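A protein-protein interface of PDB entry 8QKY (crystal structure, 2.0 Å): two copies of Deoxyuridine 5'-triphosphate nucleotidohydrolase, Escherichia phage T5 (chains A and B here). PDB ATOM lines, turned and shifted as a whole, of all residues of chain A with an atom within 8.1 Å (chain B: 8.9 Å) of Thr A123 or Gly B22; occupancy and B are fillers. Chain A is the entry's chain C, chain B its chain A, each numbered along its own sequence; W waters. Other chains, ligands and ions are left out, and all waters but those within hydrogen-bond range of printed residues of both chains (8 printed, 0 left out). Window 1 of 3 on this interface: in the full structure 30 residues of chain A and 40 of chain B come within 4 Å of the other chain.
OG of Ser B17 is in hydrogen-bond range of N of Ala B20, at 3.2 Å.
The backbone carbonyl oxygen of Met B23 lies within hydrogen-bond range of the backbone NH of Leu B115, at 2.8 Å.
The backbone carbonyl oxygen (O) of Val B65 is in hydrogen-bond range of the backbone NH (N) of Gln B114 (2.7 Å).
Printed residues of chain B within 4 Å of Thr A123: Ile B15, Ala B20, Ala B21, Gly B22 and Met B23.
Gly B22 touches just one residue of chain A: Thr A123 (3.7 Å).
No residue of chain B comes within 4 Å of Ser A122.
Ala B21 touches just these residues of chain A: Phe A61 (3.5 Å), Val A83 (3.7 Å), Asp A85 (2.7 Å), His A120 (3.7 Å) and Thr A123 (3.6 Å).
Printed residues of chain A within 4 Å of Ser B17: His A124.
Of the printed residues of chain A, Val B116 touches Phe A61 (3.7 Å).
The nearest printed residue of chain B that does not touch Thr A123 is Ser B17 (4.0004 Å).
The nearest residue of chain A that does not touch Gly B22 is Asp A85 (4.5 Å).
The nearest printed residue of chain B that does not touch Lys A127 is Met B12 (7.5 Å).
The backbone NH (N) of Ile B2 lies within hydrogen-bond range of the backbone carbonyl oxygen (O) of Asn A125.
The backbone carbonyl oxygen (O) of Ile B2 sits at hydrogen-bond distance from the backbone NH (N) of Lys A127, at 2.9 Å.
The backbone NH of Ile B4 is in hydrogen-bond range of the backbone carbonyl oxygen of Lys A127 (2.8 Å).
NE2 of His A124 sits at hydrogen-bond distance from O of Gly B16.
A ring nitrogen (NE2) of His A124 sits at hydrogen-bond distance from the backbone carbonyl oxygen (O) of Ser B17 (3.1 Å).
The backbone NH of Ala B21 lies within hydrogen-bond range of the side-chain carboxylate of Asp A85.
The backbone carbonyl oxygen (O) of Val B117 lies within hydrogen-bond range of the backbone NH (N) of Tyr A121 (2.7 Å).
No position is printed for both chains.
Of the 30 pairs that touch across the chains among the printed residues, none has its exchanged pair printed and touching as well.
Water W4 lies within hydrogen-bond range of a ring nitrogen (NE2) of His A120 (2.8 Å) and the backbone carbonyl oxygen (O) of Asp B19 (3.3 Å).
Water W3 lies within hydrogen-bond range of the side-chain hydroxyl of Ser B17 and the side-chain carboxylate of Asp A85.
Among the printed residues, pairs that only touch across the chains: Phe A126 with Ile B2, His A120 with Ala B20, His A120 with Val B117, His A124 with Glu B18, His A124 with Ile B15, Thr A123 with Ala B20, Phe A61 with Ala B21, Phe A126 with Met B12, Thr A123 with Ile B15, Asp A85 with Ala B20, Thr A123 with Ala B21, Phe A61 with Leu B118, Tyr A121 with Ile B2, Val A83 with Gln B114, Thr A123 with Gly B22, Phe A126 with Ile B15, His A120 with Ala B21, Val A83 with Ala B21, Phe A61 with Val B116, His A120 with Asp B19, Thr A123 with Met B23, Phe A126 with Ile B4 and Val A83 with Val B65.
Of the 26 printed residues of chain B, 17 touch a printed residue of chain A.
Hydrophobic or aromatic side chains of chain B within 4 Å of the printed part of chain A: Ile B2, Ile B4, Met B12, Ile B15, Ala B21, Met B23, Val B65, Val B116, Val B117 and Leu B118.
Printed residues of chain A that touch a printed residue of chain B: Phe A61, Val A83, Asp A85, His A120, Tyr A121, Thr A123, His A124, Asn A125, Phe A126 and Lys A127.
Among the printed residues, 30 pairs touch across the chains.
Among the printed residues, no Asp or Glu carboxylate lies within 4 Å of a Lys or Arg side-chain nitrogen of the other chain.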
ATOM      1  N   PHE A  61      20.874 -27.416  -6.220  1.00  0.00           N
ATOM      2  CA  PHE A  61      22.083 -28.055  -5.737  1.00  0.00           C
ATOM      3  C   PHE A  61      22.443 -27.425  -4.408  1.00  0.00           C
ATOM      4  O   PHE A  61      21.897 -26.396  -4.016  1.00  0.00           O
ATOM      5  CB  PHE A  61      23.238 -27.926  -6.736  1.00  0.00           C
ATOM      6  CG  PHE A  61      23.851 -26.550  -6.784  1.00  0.00           C
ATOM      7  CD1 PHE A  61      23.186 -25.500  -7.413  1.00  0.00           C
ATOM      8  CD2 PHE A  61      25.084 -26.301  -6.216  1.00  0.00           C
ATOM      9  CE1 PHE A  61      23.746 -24.236  -7.480  1.00  0.00           C
ATOM     10  CE2 PHE A  61      25.650 -25.020  -6.276  1.00  0.00           C
ATOM     11  CZ  PHE A  61      24.979 -23.999  -6.904  1.00  0.00           C
ATOM     12  N   VAL A  83      30.098 -28.669  -3.723  1.00  0.00           N
ATOM     13  CA  VAL A  83      28.975 -28.636  -4.647  1.00  0.00           C
ATOM     14  C   VAL A  83      28.266 -29.977  -4.522  1.00  0.00           C
ATOM     15  O   VAL A  83      28.819 -31.019  -4.906  1.00  0.00           O
ATOM     16  CB  VAL A  83      29.430 -28.376  -6.090  1.00  0.00           C
ATOM     17  CG1 VAL A  83      28.263 -28.493  -7.051  1.00  0.00           C
ATOM     18  CG2 VAL A  83      30.090 -26.998  -6.187  1.00  0.00           C
ATOM     19  N   ASP A  85      25.355 -32.253  -5.639  1.00  0.00           N
ATOM     20  CA  ASP A  85      24.352 -32.468  -6.670  1.00  0.00           C
ATOM     21  C   ASP A  85      23.099 -33.092  -6.067  1.00  0.00           C
ATOM     22  O   ASP A  85      23.131 -33.718  -5.001  1.00  0.00           O
ATOM     23  CB  ASP A  85      24.895 -33.364  -7.787  1.00  0.00           C
ATOM     24  CG  ASP A  85      26.218 -32.874  -8.336  1.00  0.00           C
ATOM     25  OD1 ASP A  85      26.228 -31.812  -8.998  1.00  0.00           O
ATOM     26  OD2 ASP A  85      27.250 -33.543  -8.094  1.00  0.00           O
ATOM     27  N   HIS A 120      20.064 -24.254 -10.348  1.00  0.00           N
ATOM     28  CA  HIS A 120      21.079 -24.253 -11.396  1.00  0.00           C
ATOM     29  C   HIS A 120      20.437 -24.522 -12.752  1.00  0.00           C
ATOM     30  O   HIS A 120      19.382 -25.155 -12.847  1.00  0.00           O
ATOM     31  CB  HIS A 120      22.175 -25.295 -11.124  1.00  0.00           C
ATOM     32  CG  HIS A 120      21.691 -26.703 -11.227  1.00  0.00           C
ATOM     33  ND1 HIS A 120      21.661 -27.394 -12.420  1.00  0.00           N
ATOM     34  CD2 HIS A 120      21.203 -27.548 -10.288  1.00  0.00           C
ATOM     35  CE1 HIS A 120      21.178 -28.608 -12.210  1.00  0.00           C
ATOM     36  NE2 HIS A 120      20.897 -28.729 -10.923  1.00  0.00           N
ATOM     37  N   TYR A 121      21.072 -24.012 -13.799  1.00  0.00           N
ATOM     38  CA  TYR A 121      20.670 -24.333 -15.160  1.00  0.00           C
ATOM     39  C   TYR A 121      20.974 -25.796 -15.457  1.00  0.00           C
ATOM     40  O   TYR A 121      21.924 -26.372 -14.925  1.00  0.00           O
ATOM     41  CB  TYR A 121      21.415 -23.430 -16.145  1.00  0.00           C
ATOM     42  CG  TYR A 121      20.642 -23.062 -17.391  1.00  0.00           C
ATOM     43  CD1 TYR A 121      19.795 -21.951 -17.409  1.00  0.00           C
ATOM     44  CD2 TYR A 121      20.782 -23.804 -18.560  1.00  0.00           C
ATOM     45  CE1 TYR A 121      19.089 -21.596 -18.561  1.00  0.00           C
ATOM     46  CE2 TYR A 121      20.084 -23.463 -19.718  1.00  0.00           C
ATOM     47  CZ  TYR A 121      19.242 -22.360 -19.710  1.00  0.00           C
ATOM     48  OH  TYR A 121      18.555 -22.025 -20.853  1.00  0.00           O
ATOM     49  N   SER A 122      20.148 -26.405 -16.303  1.00  0.00           N
ATOM     50  CA  SER A 122      20.378 -27.786 -16.712  1.00  0.00           C
ATOM     51  C   SER A 122      21.657 -27.872 -17.534  1.00  0.00           C
ATOM     52  O   SER A 122      21.781 -27.203 -18.562  1.00  0.00           O
ATOM     53  CB  SER A 122      19.196 -28.305 -17.526  1.00  0.00           C
ATOM     54  OG  SER A 122      19.595 -29.471 -18.220  1.00  0.00           O
ATOM     55  N   THR A 123      22.616 -28.683 -17.084  1.00  0.00           N
ATOM     56  CA  THR A 123      23.883 -28.732 -17.796  1.00  0.00           C
ATOM     57  C   THR A 123      23.779 -29.480 -19.114  1.00  0.00           C
ATOM     58  O   THR A 123      24.742 -29.483 -19.884  1.00  0.00           O
ATOM     59  CB  THR A 123      24.959 -29.376 -16.935  1.00  0.00           C
ATOM     60  OG1 THR A 123      24.639 -30.757 -16.735  1.00  0.00           O
ATOM     61  CG2 THR A 123      25.048 -28.659 -15.590  1.00  0.00           C
ATOM     62  N   HIS A 124      22.650 -30.111 -19.393  1.00  0.00           N
ATOM     63  CA  HIS A 124      22.469 -30.739 -20.691  1.00  0.00           C
ATOM     64  C   HIS A 124      21.859 -29.792 -21.713  1.00  0.00           C
ATOM     65  O   HIS A 124      21.869 -30.114 -22.904  1.00  0.00           O
ATOM     66  CB  HIS A 124      21.609 -32.002 -20.553  1.00  0.00           C
ATOM     67  CG  HIS A 124      22.267 -33.085 -19.760  1.00  0.00           C
ATOM     68  ND1 HIS A 124      21.834 -34.393 -19.775  1.00  0.00           N
ATOM     69  CD2 HIS A 124      23.328 -33.051 -18.921  1.00  0.00           C
ATOM     70  CE1 HIS A 124      22.605 -35.119 -18.984  1.00  0.00           C
ATOM     71  NE2 HIS A 124      23.519 -34.327 -18.452  1.00  0.00           N
ATOM     72  N   ASN A 125      21.366 -28.621 -21.291  1.00  0.00           N
ATOM     73  CA  ASN A 125      20.688 -27.695 -22.204  1.00  0.00           C
ATOM     74  C   ASN A 125      21.699 -26.689 -22.754  1.00  0.00           C
ATOM     75  O   ASN A 125      21.731 -25.506 -22.405  1.00  0.00           O
ATOM     76  CB  ASN A 125      19.521 -27.004 -21.511  1.00  0.00           C
ATOM     77  CG  ASN A 125      18.728 -26.119 -22.459  1.00  0.00           C
ATOM     78  OD1 ASN A 125      18.855 -26.237 -23.676  1.00  0.00           O
ATOM     79  ND2 ASN A 125      17.911 -25.229 -21.910  1.00  0.00           N
ATOM     80  N   PHE A 126      22.543 -27.195 -23.645  1.00  0.00           N
ATOM     81  CA  PHE A 126      23.587 -26.407 -24.268  1.00  0.00           C
ATOM     82  C   PHE A 126      23.632 -26.735 -25.749  1.00  0.00           C
ATOM     83  O   PHE A 126      23.064 -27.726 -26.208  1.00  0.00           O
ATOM     84  CB  PHE A 126      24.961 -26.675 -23.642  1.00  0.00           C
ATOM     85  CG  PHE A 126      25.478 -28.051 -23.916  1.00  0.00           C
ATOM     86  CD1 PHE A 126      26.161 -28.339 -25.094  1.00  0.00           C
ATOM     87  CD2 PHE A 126      25.259 -29.073 -23.005  1.00  0.00           C
ATOM     88  CE1 PHE A 126      26.620 -29.619 -25.353  1.00  0.00           C
ATOM     89  CE2 PHE A 126      25.721 -30.351 -23.254  1.00  0.00           C
ATOM     90  CZ  PHE A 126      26.404 -30.624 -24.428  1.00  0.00           C
ATOM     91  N   LYS A 127      24.361 -25.907 -26.487  1.00  0.00           N
ATOM     92  CA  LYS A 127      24.586 -26.117 -27.907  1.00  0.00           C
ATOM     93  C   LYS A 127      25.985 -25.612 -28.226  1.00  0.00           C
ATOM     94  O   LYS A 127      26.346 -24.507 -27.816  1.00  0.00           O
ATOM     95  CB  LYS A 127      23.529 -25.375 -28.739  1.00  0.00           C
ATOM     96  CG  LYS A 127      23.739 -25.442 -30.240  1.00  0.00           C
ATOM     97  CD  LYS A 127      22.637 -24.701 -30.980  1.00  0.00           C
ATOM     98  CE  LYS A 127      22.670 -25.030 -32.467  1.00  0.00           C
ATOM     99  NZ  LYS A 127      21.601 -24.304 -33.216  1.00  0.00           N
ATOM    100  N   ILE B   2      22.401 -22.639 -23.022  1.00  0.00           N
ATOM    101  CA  ILE B   2      23.765 -22.125 -22.977  1.00  0.00           C
ATOM    102  C   ILE B   2      24.422 -22.415 -24.316  1.00  0.00           C
ATOM    103  O   ILE B   2      24.410 -23.557 -24.789  1.00  0.00           O
ATOM    104  CB  ILE B   2      24.562 -22.773 -21.836  1.00  0.00           C
ATOM    105  CG1 ILE B   2      24.008 -22.386 -20.468  1.00  0.00           C
ATOM    106  CG2 ILE B   2      26.026 -22.335 -21.884  1.00  0.00           C
ATOM    107  CD1 ILE B   2      24.284 -23.474 -19.429  1.00  0.00           C
ATOM    108  N   ILE B   4      27.964 -22.633 -26.410  1.00  0.00           N
ATOM    109  CA  ILE B   4      29.354 -22.911 -26.065  1.00  0.00           C
ATOM    110  C   ILE B   4      30.214 -22.878 -27.327  1.00  0.00           C
ATOM    111  O   ILE B   4      29.899 -23.543 -28.320  1.00  0.00           O
ATOM    112  CB  ILE B   4      29.499 -24.274 -25.363  1.00  0.00           C
ATOM    113  CG1 ILE B   4      28.631 -24.341 -24.104  1.00  0.00           C
ATOM    114  CG2 ILE B   4      30.942 -24.531 -25.039  1.00  0.00           C
ATOM    115  CD1 ILE B   4      28.681 -25.709 -23.417  1.00  0.00           C
ATOM    116  N   MET B  12      35.771 -29.603 -24.757  1.00  0.00           N
ATOM    117  CA  MET B  12      34.379 -29.759 -24.354  1.00  0.00           C
ATOM    118  C   MET B  12      34.275 -30.059 -22.862  1.00  0.00           C
ATOM    119  O   MET B  12      34.854 -31.054 -22.396  1.00  0.00           O
ATOM    120  CB  MET B  12      33.721 -30.884 -25.140  1.00  0.00           C
ATOM    121  CG  MET B  12      32.373 -31.238 -24.595  1.00  0.00           C
ATOM    122  SD  MET B  12      31.205 -29.908 -24.933  1.00  0.00           S
ATOM    123  CE  MET B  12      29.848 -30.356 -23.852  1.00  0.00           C
ATOM    124  N   PRO B  13      33.567 -29.240 -22.087  1.00  0.00           N
ATOM    125  CA  PRO B  13      33.424 -29.543 -20.657  1.00  0.00           C
ATOM    126  C   PRO B  13      32.806 -30.918 -20.429  1.00  0.00           C
ATOM    127  O   PRO B  13      31.946 -31.371 -21.188  1.00  0.00           O
ATOM    128  CB  PRO B  13      32.507 -28.427 -20.143  1.00  0.00           C
ATOM    129  CG  PRO B  13      32.734 -27.274 -21.119  1.00  0.00           C
ATOM    130  CD  PRO B  13      32.922 -27.959 -22.454  1.00  0.00           C
ATOM    131  N   LYS B  14      33.254 -31.580 -19.361  1.00  0.00           N
ATOM    132  CA  LYS B  14      32.693 -32.881 -18.991  1.00  0.00           C
ATOM    133  C   LYS B  14      31.266 -32.706 -18.481  1.00  0.00           C
ATOM    134  O   LYS B  14      31.039 -32.092 -17.433  1.00  0.00           O
ATOM    135  CB  LYS B  14      33.553 -33.557 -17.926  1.00  0.00           C
ATOM    136  CG  LYS B  14      33.156 -35.019 -17.646  1.00  0.00           C
ATOM    137  CD  LYS B  14      33.084 -35.822 -18.944  1.00  0.00           C
ATOM    138  CE  LYS B  14      32.657 -37.275 -18.713  1.00  0.00           C
ATOM    139  NZ  LYS B  14      33.545 -38.204 -19.492  1.00  0.00           N
ATOM    140  N   ILE B  15      30.306 -33.262 -19.208  1.00  0.00           N
ATOM    141  CA  ILE B  15      28.899 -33.199 -18.830  1.00  0.00           C
ATOM    142  C   ILE B  15      28.582 -34.410 -17.976  1.00  0.00           C
ATOM    143  O   ILE B  15      28.960 -35.531 -18.321  1.00  0.00           O
ATOM    144  CB  ILE B  15      27.999 -33.159 -20.077  1.00  0.00           C
ATOM    145  CG1 ILE B  15      28.401 -31.991 -20.979  1.00  0.00           C
ATOM    146  CG2 ILE B  15      26.556 -33.042 -19.682  1.00  0.00           C
ATOM    147  CD1 ILE B  15      28.039 -30.639 -20.412  1.00  0.00           C
ATOM    148  N   GLY B  16      27.895 -34.193 -16.859  1.00  0.00           N
ATOM    149  CA  GLY B  16      27.544 -35.254 -15.947  1.00  0.00           C
ATOM    150  C   GLY B  16      26.113 -35.714 -16.121  1.00  0.00           C
ATOM    151  O   GLY B  16      25.507 -35.580 -17.189  1.00  0.00           O
ATOM    152  N   SER B  17      25.559 -36.248 -15.037  1.00  0.00           N
ATOM    153  CA  SER B  17      24.176 -36.694 -15.033  1.00  0.00           C
ATOM    154  C   SER B  17      23.242 -35.522 -15.314  1.00  0.00           C
ATOM    155  O   SER B  17      23.640 -34.357 -15.305  1.00  0.00           O
ATOM    156  CB  SER B  17      23.842 -37.348 -13.690  1.00  0.00           C
ATOM    157  OG  SER B  17      23.644 -36.365 -12.686  1.00  0.00           O
ATOM    158  N   GLU B  18      21.976 -35.842 -15.585  1.00  0.00           N
ATOM    159  CA  GLU B  18      20.986 -34.782 -15.758  1.00  0.00           C
ATOM    160  C   GLU B  18      20.783 -33.979 -14.480  1.00  0.00           C
ATOM    161  O   GLU B  18      20.300 -32.843 -14.543  1.00  0.00           O
ATOM    162  CB  GLU B  18      19.646 -35.365 -16.221  1.00  0.00           C
ATOM    163  CG  GLU B  18      19.439 -35.308 -17.733  1.00  0.00           C
ATOM    164  CD  GLU B  18      18.248 -36.135 -18.219  1.00  0.00           C
ATOM    165  OE1 GLU B  18      18.376 -36.785 -19.283  1.00  0.00           O
ATOM    166  OE2 GLU B  18      17.190 -36.127 -17.549  1.00  0.00           O
ATOM    167  N   ASP B  19      21.142 -34.544 -13.328  1.00  0.00           N
ATOM    168  CA  ASP B  19      21.041 -33.852 -12.051  1.00  0.00           C
ATOM    169  C   ASP B  19      22.262 -33.002 -11.723  1.00  0.00           C
ATOM    170  O   ASP B  19      22.201 -32.223 -10.767  1.00  0.00           O
ATOM    171  CB  ASP B  19      20.844 -34.868 -10.925  1.00  0.00           C
ATOM    172  CG  ASP B  19      19.509 -35.564 -11.001  1.00  0.00           C
ATOM    173  OD1 ASP B  19      18.510 -34.896 -11.347  1.00  0.00           O
ATOM    174  OD2 ASP B  19      19.466 -36.784 -10.731  1.00  0.00           O
ATOM    175  N   ALA B  20      23.360 -33.145 -12.470  1.00  0.00           N
ATOM    176  CA  ALA B  20      24.608 -32.458 -12.144  1.00  0.00           C
ATOM    177  C   ALA B  20      24.406 -30.951 -12.023  1.00  0.00           C
ATOM    178  O   ALA B  20      23.756 -30.327 -12.861  1.00  0.00           O
ATOM    179  CB  ALA B  20      25.664 -32.755 -13.209  1.00  0.00           C
ATOM    180  N   ALA B  21      24.961 -30.367 -10.961  1.00  0.00           N
ATOM    181  CA  ALA B  21      24.902 -28.915 -10.805  1.00  0.00           C
ATOM    182  C   ALA B  21      25.719 -28.208 -11.881  1.00  0.00           C
ATOM    183  O   ALA B  21      25.353 -27.118 -12.336  1.00  0.00           O
ATOM    184  CB  ALA B  21      25.403 -28.525  -9.415  1.00  0.00           C
ATOM    185  N   GLY B  22      26.834 -28.800 -12.294  1.00  0.00           N
ATOM    186  CA  GLY B  22      27.736 -28.098 -13.181  1.00  0.00           C
ATOM    187  C   GLY B  22      28.400 -29.042 -14.156  1.00  0.00           C
ATOM    188  O   GLY B  22      28.134 -30.241 -14.171  1.00  0.00           O
ATOM    189  N   MET B  23      29.250 -28.472 -14.998  1.00  0.00           N
ATOM    190  CA  MET B  23      30.067 -29.214 -15.945  1.00  0.00           C
ATOM    191  C   MET B  23      31.527 -28.905 -15.655  1.00  0.00           C
ATOM    192  O   MET B  23      31.856 -27.825 -15.159  1.00  0.00           O
ATOM    193  CB  MET B  23      29.720 -28.843 -17.406  1.00  0.00           C
ATOM    194  CG  MET B  23      29.640 -27.350 -17.631  1.00  0.00           C
ATOM    195  SD  MET B  23      29.264 -26.848 -19.333  1.00  0.00           S
ATOM    196  CE  MET B  23      27.478 -27.017 -19.252  1.00  0.00           C
ATOM    197  N   ASP B  24      32.402 -29.866 -15.938  1.00  0.00           N
ATOM    198  CA  ASP B  24      33.810 -29.743 -15.583  1.00  0.00           C
ATOM    199  C   ASP B  24      34.563 -29.008 -16.688  1.00  0.00           C
ATOM    200  O   ASP B  24      34.607 -29.481 -17.827  1.00  0.00           O
ATOM    201  CB  ASP B  24      34.429 -31.124 -15.354  1.00  0.00           C
ATOM    202  CG  ASP B  24      34.069 -31.716 -13.997  1.00  0.00           C
ATOM    203  OD1 ASP B  24      33.394 -31.028 -13.195  1.00  0.00           O
ATOM    204  OD2 ASP B  24      34.481 -32.872 -13.727  1.00  0.00           O
ATOM    205  N   LEU B  25      35.181 -27.878 -16.350  1.00  0.00           N
ATOM    206  CA  LEU B  25      36.087 -27.205 -17.271  1.00  0.00           C
ATOM    207  C   LEU B  25      37.461 -27.867 -17.234  1.00  0.00           C
ATOM    208  O   LEU B  25      37.934 -28.285 -16.175  1.00  0.00           O
ATOM    209  CB  LEU B  25      36.206 -25.715 -16.926  1.00  0.00           C
ATOM    210  CG  LEU B  25      34.882 -24.944 -16.935  1.00  0.00           C
ATOM    211  CD1 LEU B  25      35.002 -23.599 -16.226  1.00  0.00           C
ATOM    212  CD2 LEU B  25      34.415 -24.748 -18.359  1.00  0.00           C
ATOM    213  N   LEU B  63      29.302 -19.608 -12.149  1.00  0.00           N
ATOM    214  CA  LEU B  63      30.163 -19.689 -10.977  1.00  0.00           C
ATOM    215  C   LEU B  63      31.176 -20.796 -11.223  1.00  0.00           C
ATOM    216  O   LEU B  63      30.791 -21.927 -11.532  1.00  0.00           O
ATOM    217  CB  LEU B  63      29.341 -19.968  -9.721  1.00  0.00           C
ATOM    218  CG  LEU B  63      30.081 -20.012  -8.394  1.00  0.00           C
ATOM    219  CD1 LEU B  63      30.538 -18.608  -8.053  1.00  0.00           C
ATOM    220  CD2 LEU B  63      29.161 -20.572  -7.317  1.00  0.00           C
ATOM    221  N   VAL B  65      34.215 -22.930  -9.588  1.00  0.00           N
ATOM    222  CA  VAL B  65      34.873 -23.340  -8.349  1.00  0.00           C
ATOM    223  C   VAL B  65      35.684 -24.595  -8.646  1.00  0.00           C
ATOM    224  O   VAL B  65      35.426 -25.287  -9.643  1.00  0.00           O
ATOM    225  CB  VAL B  65      33.846 -23.604  -7.224  1.00  0.00           C
ATOM    226  CG1 VAL B  65      33.097 -22.329  -6.873  1.00  0.00           C
ATOM    227  CG2 VAL B  65      32.865 -24.686  -7.662  1.00  0.00           C
ATOM    228  N   ARG B  67      37.013 -28.389  -8.740  1.00  0.00           N
ATOM    229  CA  ARG B  67      36.507 -29.732  -8.504  1.00  0.00           C
ATOM    230  C   ARG B  67      36.929 -30.205  -7.117  1.00  0.00           C
ATOM    231  O   ARG B  67      37.926 -29.748  -6.553  1.00  0.00           O
ATOM    232  CB  ARG B  67      37.026 -30.701  -9.569  1.00  0.00           C
ATOM    233  CG  ARG B  67      36.349 -30.539 -10.917  1.00  0.00           C
ATOM    234  CD  ARG B  67      36.865 -31.589 -11.910  1.00  0.00           C
ATOM    235  NE  ARG B  67      36.287 -32.900 -11.648  1.00  0.00           N
ATOM    236  CZ  ARG B  67      36.985 -34.018 -11.535  1.00  0.00           C
ATOM    237  NH1 ARG B  67      38.299 -34.028 -11.683  1.00  0.00           N
ATOM    238  NH2 ARG B  67      36.350 -35.154 -11.264  1.00  0.00           N
ATOM    239  N   ARG B 111      40.243 -32.404 -16.290  1.00  0.00           N
ATOM    240  CA  ARG B 111      39.142 -31.688 -15.657  1.00  0.00           C
ATOM    241  C   ARG B 111      39.599 -31.011 -14.366  1.00  0.00           C
ATOM    242  O   ARG B 111      40.163 -31.665 -13.483  1.00  0.00           O
ATOM    243  CB  ARG B 111      38.005 -32.663 -15.371  1.00  0.00           C
ATOM    244  CG  ARG B 111      37.388 -33.247 -16.629  1.00  0.00           C
ATOM    245  CD  ARG B 111      36.811 -34.638 -16.388  1.00  0.00           C
ATOM    246  NE  ARG B 111      35.749 -34.644 -15.391  1.00  0.00           N
ATOM    247  CZ  ARG B 111      35.233 -35.743 -14.855  1.00  0.00           C
ATOM    248  NH1 ARG B 111      35.658 -36.946 -15.204  1.00  0.00           N
ATOM    249  NH2 ARG B 111      34.262 -35.633 -13.949  1.00  0.00           N
ATOM    250  N   CYS B 113      37.934 -27.536 -12.863  1.00  0.00           N
ATOM    251  CA  CYS B 113      36.976 -26.701 -12.160  1.00  0.00           C
ATOM    252  C   CYS B 113      35.571 -27.038 -12.621  1.00  0.00           C
ATOM    253  O   CYS B 113      35.364 -27.539 -13.725  1.00  0.00           O
ATOM    254  CB  CYS B 113      37.245 -25.201 -12.399  1.00  0.00           C
ATOM    255  SG  CYS B 113      38.742 -24.596 -11.573  1.00  0.00           S
ATOM    256  N   GLN B 114      34.609 -26.756 -11.752  1.00  0.00           N
ATOM    257  CA  GLN B 114      33.196 -26.856 -12.078  1.00  0.00           C
ATOM    258  C   GLN B 114      32.665 -25.496 -12.533  1.00  0.00           C
ATOM    259  O   GLN B 114      32.965 -24.469 -11.920  1.00  0.00           O
ATOM    260  CB  GLN B 114      32.413 -27.312 -10.849  1.00  0.00           C
ATOM    261  CG  GLN B 114      32.651 -28.745 -10.429  1.00  0.00           C
ATOM    262  CD  GLN B 114      31.412 -29.346  -9.800  1.00  0.00           C
ATOM    263  OE1 GLN B 114      30.323 -29.310 -10.382  1.00  0.00           O
ATOM    264  NE2 GLN B 114      31.568 -29.906  -8.618  1.00  0.00           N
ATOM    265  N   LEU B 115      31.862 -25.498 -13.593  1.00  0.00           N
ATOM    266  CA  LEU B 115      31.098 -24.323 -14.021  1.00  0.00           C
ATOM    267  C   LEU B 115      29.641 -24.593 -13.674  1.00  0.00           C
ATOM    268  O   LEU B 115      29.036 -25.519 -14.216  1.00  0.00           O
ATOM    269  CB  LEU B 115      31.251 -24.051 -15.521  1.00  0.00           C
ATOM    270  CG  LEU B 115      30.254 -23.049 -16.116  1.00  0.00           C
ATOM    271  CD1 LEU B 115      30.497 -21.638 -15.545  1.00  0.00           C
ATOM    272  CD2 LEU B 115      30.271 -23.022 -17.658  1.00  0.00           C
ATOM    273  N   VAL B 116      29.085 -23.802 -12.764  1.00  0.00           N
ATOM    274  CA  VAL B 116      27.682 -23.894 -12.382  1.00  0.00           C
ATOM    275  C   VAL B 116      26.988 -22.629 -12.868  1.00  0.00           C
ATOM    276  O   VAL B 116      27.491 -21.523 -12.652  1.00  0.00           O
ATOM    277  CB  VAL B 116      27.520 -24.050 -10.859  1.00  0.00           C
ATOM    278  CG1 VAL B 116      26.039 -24.095 -10.481  1.00  0.00           C
ATOM    279  CG2 VAL B 116      28.275 -25.301 -10.326  1.00  0.00           C
ATOM    280  N   VAL B 117      25.843 -22.776 -13.523  1.00  0.00           N
ATOM    281  CA  VAL B 117      25.113 -21.626 -14.053  1.00  0.00           C
ATOM    282  C   VAL B 117      23.884 -21.422 -13.171  1.00  0.00           C
ATOM    283  O   VAL B 117      23.057 -22.334 -13.032  1.00  0.00           O
ATOM    284  CB  VAL B 117      24.734 -21.823 -15.534  1.00  0.00           C
ATOM    285  CG1 VAL B 117      23.890 -20.650 -16.048  1.00  0.00           C
ATOM    286  CG2 VAL B 117      25.993 -21.976 -16.412  1.00  0.00           C
ATOM    287  N   LEU B 118      23.768 -20.236 -12.576  1.00  0.00           N
ATOM    288  CA  LEU B 118      22.789 -19.895 -11.553  1.00  0.00           C
ATOM    289  C   LEU B 118      22.168 -18.542 -11.856  1.00  0.00           C
ATOM    290  O   LEU B 118      22.804 -17.695 -12.487  1.00  0.00           O
ATOM    291  CB  LEU B 118      23.410 -19.793 -10.151  1.00  0.00           C
ATOM    292  CG  LEU B 118      24.422 -20.724  -9.538  1.00  0.00           C
ATOM    293  CD1 LEU B 118      25.794 -20.258  -9.928  1.00  0.00           C
ATOM    294  CD2 LEU B 118      24.230 -20.645  -8.029  1.00  0.00           C
HETATM  295  O   HOH W   1      28.250 -31.083 -10.532  1.00  0.00           O
HETATM  296  O   HOH W   2      29.541 -32.061  -7.336  1.00  0.00           O
HETATM  297  O   HOH W   3      25.624 -35.516 -10.229  1.00  0.00           O
HETATM  298  O   HOH W   4      19.283 -30.873 -10.246  1.00  0.00           O
HETATM  299  O   HOH W   5      27.304 -31.692 -16.331  1.00  0.00           O
HETATM  300  O   HOH W   6      22.378 -30.672 -15.031  1.00  0.00           O
HETATM  301  O   HOH W   7      22.333 -30.709  -8.636  1.00  0.00           O
HETATM  302  O   HOH W   8      24.512 -25.351 -14.155  1.00  0.00           O
